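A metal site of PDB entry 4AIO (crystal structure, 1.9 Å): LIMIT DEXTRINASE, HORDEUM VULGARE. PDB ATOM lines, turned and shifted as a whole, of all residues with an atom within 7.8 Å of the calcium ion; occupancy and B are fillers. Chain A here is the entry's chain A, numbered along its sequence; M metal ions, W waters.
ND2 of Asn 700 sits at hydrogen-bond distance from OE2 of Glu 348.
Four residues have an atom within 4 Å of the calcium ion: Gln 347, Asp 350, Tyr 352 and Asn 700.
The nearest printed residue that does not touch the calcium ion is Gly 313 (4.3 Å).
The calcium ion is bound by the backbone carbonyl oxygen (O) of Gln 347.
The backbone carbonyl oxygen (O) of Tyr 352 binds the calcium ion, at 2.3 Å.
The calcium ion is bound by the side-chain carboxylate (OD1) of Asp 350 (2.4 Å).
The calcium ion is bound by water W2 (2.4 Å).
The calcium ion is bound by OD1 of Asn 700 (2.4 Å).
Water W3 binds the calcium ion, 2.5 Å away.
The calcium ion is bound by water W1 (2.5 Å).
The calcium ion has seven donor atoms within binding distance.
Water W3 bridges O of Gly 313 (2.6 Å) and ND2 of Asn 353 (3.2 Å).
Water W2 lies within hydrogen-bond range of OD2 of Asp 350 (2.7 Å), O of Asn 700 (2.8 Å) and N of Gly 702 (3.5 Å).
Water W1 lies within hydrogen-bond range of the backbone carbonyl oxygen of Asp 350 (2.6 Å) and the backbone carbonyl oxygen of Gly 313 (2.8 Å).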
ATOM      1  N   GLY A 313     -12.035  12.270   4.027  1.00  0.00           N
ATOM      2  CA  GLY A 313     -13.461  11.990   4.190  1.00  0.00           C
ATOM      3  C   GLY A 313     -14.343  13.170   3.871  1.00  0.00           C
ATOM      4  O   GLY A 313     -15.553  13.014   3.804  1.00  0.00           O
ATOM      5  N   VAL A 314     -13.745  14.354   3.709  1.00  0.00           N
ATOM      6  CA  VAL A 314     -14.448  15.539   3.199  1.00  0.00           C
ATOM      7  C   VAL A 314     -13.608  16.138   2.078  1.00  0.00           C
ATOM      8  O   VAL A 314     -12.398  16.379   2.253  1.00  0.00           O
ATOM      9  CB  VAL A 314     -14.674  16.609   4.305  1.00  0.00           C
ATOM     10  CG1 VAL A 314     -15.407  17.825   3.705  1.00  0.00           C
ATOM     11  CG2 VAL A 314     -15.453  16.048   5.485  1.00  0.00           C
ATOM     12  N   VAL A 343     -29.633  11.142   4.298  1.00  0.00           N
ATOM     13  CA  VAL A 343     -28.278  11.491   4.760  1.00  0.00           C
ATOM     14  C   VAL A 343     -27.256  10.418   4.356  1.00  0.00           C
ATOM     15  O   VAL A 343     -26.181  10.750   3.841  1.00  0.00           O
ATOM     16  CB  VAL A 343     -28.264  11.712   6.299  1.00  0.00           C
ATOM     17  CG1 VAL A 343     -26.842  11.871   6.817  1.00  0.00           C
ATOM     18  CG2 VAL A 343     -29.099  12.940   6.661  1.00  0.00           C
ATOM     19  N   ILE A 346     -25.831  10.297   0.747  1.00  0.00           N
ATOM     20  CA  ILE A 346     -24.797  11.278   0.336  1.00  0.00           C
ATOM     21  C   ILE A 346     -23.649  11.456   1.357  1.00  0.00           C
ATOM     22  O   ILE A 346     -22.775  12.299   1.175  1.00  0.00           O
ATOM     23  CB  ILE A 346     -25.395  12.673   0.050  1.00  0.00           C
ATOM     24  CG1 ILE A 346     -26.085  13.229   1.311  1.00  0.00           C
ATOM     25  CG2 ILE A 346     -26.348  12.614  -1.130  1.00  0.00           C
ATOM     26  CD1 ILE A 346     -26.279  14.721   1.313  1.00  0.00           C
ATOM     27  N   GLN A 347     -23.659  10.666   2.434  1.00  0.00           N
ATOM     28  CA  GLN A 347     -22.715  10.896   3.542  1.00  0.00           C
ATOM     29  C   GLN A 347     -21.237  10.811   3.139  1.00  0.00           C
ATOM     30  O   GLN A 347     -20.396  11.434   3.774  1.00  0.00           O
ATOM     31  CB  GLN A 347     -23.016   9.979   4.740  1.00  0.00           C
ATOM     32  CG  GLN A 347     -22.653   8.511   4.536  1.00  0.00           C
ATOM     33  CD  GLN A 347     -23.089   7.630   5.701  1.00  0.00           C
ATOM     34  OE1 GLN A 347     -23.519   8.120   6.753  1.00  0.00           O
ATOM     35  NE2 GLN A 347     -22.954   6.339   5.526  1.00  0.00           N
ATOM     36  N   GLU A 348     -20.910  10.068   2.078  1.00  0.00           N
ATOM     37  CA  GLU A 348     -19.519   9.979   1.627  1.00  0.00           C
ATOM     38  C   GLU A 348     -19.084  11.194   0.802  1.00  0.00           C
ATOM     39  O   GLU A 348     -17.896  11.362   0.511  1.00  0.00           O
ATOM     40  CB  GLU A 348     -19.288   8.691   0.824  1.00  0.00           C
ATOM     41  CG  GLU A 348     -19.493   7.401   1.600  1.00  0.00           C
ATOM     42  CD  GLU A 348     -18.542   7.282   2.783  1.00  0.00           C
ATOM     43  OE1 GLU A 348     -17.316   7.429   2.585  1.00  0.00           O
ATOM     44  OE2 GLU A 348     -19.018   7.035   3.908  1.00  0.00           O
ATOM     45  N   GLU A 349     -20.039  12.043   0.444  1.00  0.00           N
ATOM     46  CA  GLU A 349     -19.788  13.145  -0.486  1.00  0.00           C
ATOM     47  C   GLU A 349     -20.305  14.472   0.035  1.00  0.00           C
ATOM     48  O   GLU A 349     -20.329  15.458  -0.698  1.00  0.00           O
ATOM     49  CB  GLU A 349     -20.427  12.818  -1.846  1.00  0.00           C
ATOM     50  CG  GLU A 349     -19.712  11.700  -2.596  1.00  0.00           C
ATOM     51  CD  GLU A 349     -20.659  10.749  -3.323  1.00  0.00           C
ATOM     52  OE1 GLU A 349     -21.541  11.229  -4.084  1.00  0.00           O
ATOM     53  OE2 GLU A 349     -20.522   9.522  -3.132  1.00  0.00           O
ATOM     54  N   ASP A 350     -20.732  14.479   1.284  1.00  0.00           N
ATOM     55  CA  ASP A 350     -21.278  15.695   1.891  1.00  0.00           C
ATOM     56  C   ASP A 350     -20.134  16.487   2.568  1.00  0.00           C
ATOM     57  O   ASP A 350     -18.982  16.059   2.527  1.00  0.00           O
ATOM     58  CB  ASP A 350     -22.458  15.352   2.830  1.00  0.00           C
ATOM     59  CG  ASP A 350     -22.021  14.727   4.166  1.00  0.00           C
ATOM     60  OD1 ASP A 350     -20.817  14.446   4.359  1.00  0.00           O
ATOM     61  OD2 ASP A 350     -22.912  14.561   5.039  1.00  0.00           O
ATOM     62  N   PRO A 351     -20.445  17.660   3.166  1.00  0.00           N
ATOM     63  CA  PRO A 351     -19.365  18.463   3.719  1.00  0.00           C
ATOM     64  C   PRO A 351     -18.914  18.025   5.121  1.00  0.00           C
ATOM     65  O   PRO A 351     -18.118  18.746   5.749  1.00  0.00           O
ATOM     66  CB  PRO A 351     -19.972  19.868   3.825  1.00  0.00           C
ATOM     67  CG  PRO A 351     -21.288  19.807   3.109  1.00  0.00           C
ATOM     68  CD  PRO A 351     -21.723  18.381   3.196  1.00  0.00           C
ATOM     69  N   TYR A 352     -19.411  16.888   5.613  1.00  0.00           N
ATOM     70  CA  TYR A 352     -19.368  16.587   7.045  1.00  0.00           C
ATOM     71  C   TYR A 352     -18.518  15.388   7.450  1.00  0.00           C
ATOM     72  O   TYR A 352     -18.692  14.293   6.911  1.00  0.00           O
ATOM     73  CB  TYR A 352     -20.791  16.362   7.603  1.00  0.00           C
ATOM     74  CG  TYR A 352     -20.812  16.478   9.096  1.00  0.00           C
ATOM     75  CD1 TYR A 352     -20.513  15.383   9.914  1.00  0.00           C
ATOM     76  CD2 TYR A 352     -21.075  17.701   9.705  1.00  0.00           C
ATOM     77  CE1 TYR A 352     -20.493  15.508  11.303  1.00  0.00           C
ATOM     78  CE2 TYR A 352     -21.044  17.840  11.080  1.00  0.00           C
ATOM     79  CZ  TYR A 352     -20.762  16.747  11.872  1.00  0.00           C
ATOM     80  OH  TYR A 352     -20.752  16.915  13.229  1.00  0.00           O
ATOM     81  N   ASN A 353     -17.643  15.581   8.426  1.00  0.00           N
ATOM     82  CA  ASN A 353     -17.029  14.474   9.173  1.00  0.00           C
ATOM     83  C   ASN A 353     -16.367  15.019  10.434  1.00  0.00           C
ATOM     84  O   ASN A 353     -15.860  16.147  10.418  1.00  0.00           O
ATOM     85  CB  ASN A 353     -15.982  13.749   8.308  1.00  0.00           C
ATOM     86  CG  ASN A 353     -15.613  12.377   8.844  1.00  0.00           C
ATOM     87  OD1 ASN A 353     -14.875  12.254   9.831  1.00  0.00           O
ATOM     88  ND2 ASN A 353     -16.124  11.327   8.199  1.00  0.00           N
ATOM     89  N   TRP A 354     -16.360  14.252  11.517  1.00  0.00           N
ATOM     90  CA  TRP A 354     -15.641  14.671  12.728  1.00  0.00           C
ATOM     91  C   TRP A 354     -14.213  14.937  12.420  1.00  0.00           C
ATOM     92  O   TRP A 354     -13.597  15.845  12.981  1.00  0.00           O
ATOM     93  CB  TRP A 354     -15.718  13.626  13.831  1.00  0.00           C
ATOM     94  CG  TRP A 354     -17.037  13.544  14.567  1.00  0.00           C
ATOM     95  CD1 TRP A 354     -18.085  14.462  14.546  1.00  0.00           C
ATOM     96  CD2 TRP A 354     -17.454  12.500  15.498  1.00  0.00           C
ATOM     97  NE1 TRP A 354     -19.117  14.044  15.372  1.00  0.00           N
ATOM     98  CE2 TRP A 354     -18.797  12.872  15.970  1.00  0.00           C
ATOM     99  CE3 TRP A 354     -16.885  11.314  15.946  1.00  0.00           C
ATOM    100  CZ2 TRP A 354     -19.504  12.082  16.852  1.00  0.00           C
ATOM    101  CZ3 TRP A 354     -17.622  10.520  16.828  1.00  0.00           C
ATOM    102  CH2 TRP A 354     -18.887  10.896  17.273  1.00  0.00           C
ATOM    103  N   TYR A 699     -20.454  10.663  13.798  1.00  0.00           N
ATOM    104  CA  TYR A 699     -19.273  11.073  13.023  1.00  0.00           C
ATOM    105  C   TYR A 699     -19.509  11.363  11.529  1.00  0.00           C
ATOM    106  O   TYR A 699     -18.851  12.244  10.953  1.00  0.00           O
ATOM    107  CB  TYR A 699     -18.131  10.049  13.172  1.00  0.00           C
ATOM    108  CG  TYR A 699     -18.264   8.815  12.294  1.00  0.00           C
ATOM    109  CD1 TYR A 699     -19.184   7.812  12.617  1.00  0.00           C
ATOM    110  CD2 TYR A 699     -17.477   8.658  11.152  1.00  0.00           C
ATOM    111  CE1 TYR A 699     -19.323   6.686  11.819  1.00  0.00           C
ATOM    112  CE2 TYR A 699     -17.611   7.519  10.354  1.00  0.00           C
ATOM    113  CZ  TYR A 699     -18.537   6.551  10.698  1.00  0.00           C
ATOM    114  OH  TYR A 699     -18.685   5.429   9.905  1.00  0.00           O
ATOM    115  N   ASN A 700     -20.407  10.605  10.917  1.00  0.00           N
ATOM    116  CA  ASN A 700     -20.694  10.713   9.492  1.00  0.00           C
ATOM    117  C   ASN A 700     -22.189  10.962   9.245  1.00  0.00           C
ATOM    118  O   ASN A 700     -22.710  10.670   8.150  1.00  0.00           O
ATOM    119  CB  ASN A 700     -20.215   9.444   8.770  1.00  0.00           C
ATOM    120  CG  ASN A 700     -19.826   9.681   7.305  1.00  0.00           C
ATOM    121  OD1 ASN A 700     -19.594  10.815   6.875  1.00  0.00           O
ATOM    122  ND2 ASN A 700     -19.746   8.596   6.526  1.00  0.00           N
ATOM    123  N   SER A 701     -22.874  11.537  10.242  1.00  0.00           N
ATOM    124  CA  SER A 701     -24.337  11.726  10.188  1.00  0.00           C
ATOM    125  C   SER A 701     -24.787  13.092   9.653  1.00  0.00           C
ATOM    126  O   SER A 701     -25.968  13.443   9.754  1.00  0.00           O
ATOM    127  CB  SER A 701     -24.965  11.474  11.562  1.00  0.00           C
ATOM    128  OG  SER A 701     -24.695  10.171  12.053  1.00  0.00           O
ATOM    129  N   GLY A 702     -23.839  13.859   9.111  1.00  0.00           N
ATOM    130  CA  GLY A 702     -24.105  15.136   8.450  1.00  0.00           C
ATOM    131  C   GLY A 702     -24.534  16.268   9.359  1.00  0.00           C
ATOM    132  O   GLY A 702     -24.626  16.106  10.595  1.00  0.00           O
ATOM    133  N   ASP A 703     -24.766  17.426   8.746  1.00  0.00           N
ATOM    134  CA  ASP A 703     -25.305  18.611   9.410  1.00  0.00           C
ATOM    135  C   ASP A 703     -26.691  18.345  10.017  1.00  0.00           C
ATOM    136  O   ASP A 703     -27.072  18.967  11.014  1.00  0.00           O
ATOM    137  CB  ASP A 703     -25.410  19.800   8.428  1.00  0.00           C
ATOM    138  CG  ASP A 703     -24.032  20.259   7.890  1.00  0.00           C
ATOM    139  OD1 ASP A 703     -23.019  20.157   8.600  1.00  0.00           O
ATOM    140  OD2 ASP A 703     -23.983  20.754   6.736  1.00  0.00           O
HETATM  141 CA    CA M   1     -19.568  12.746   5.451  1.00  0.00          CA
HETATM  142  O   HOH W   1     -18.237  13.821   3.615  1.00  0.00           O
HETATM  143  O   HOH W   2     -21.649  12.791   6.623  1.00  0.00           O
HETATM  144  O   HOH W   3     -17.294  11.726   5.298  1.00  0.00           O
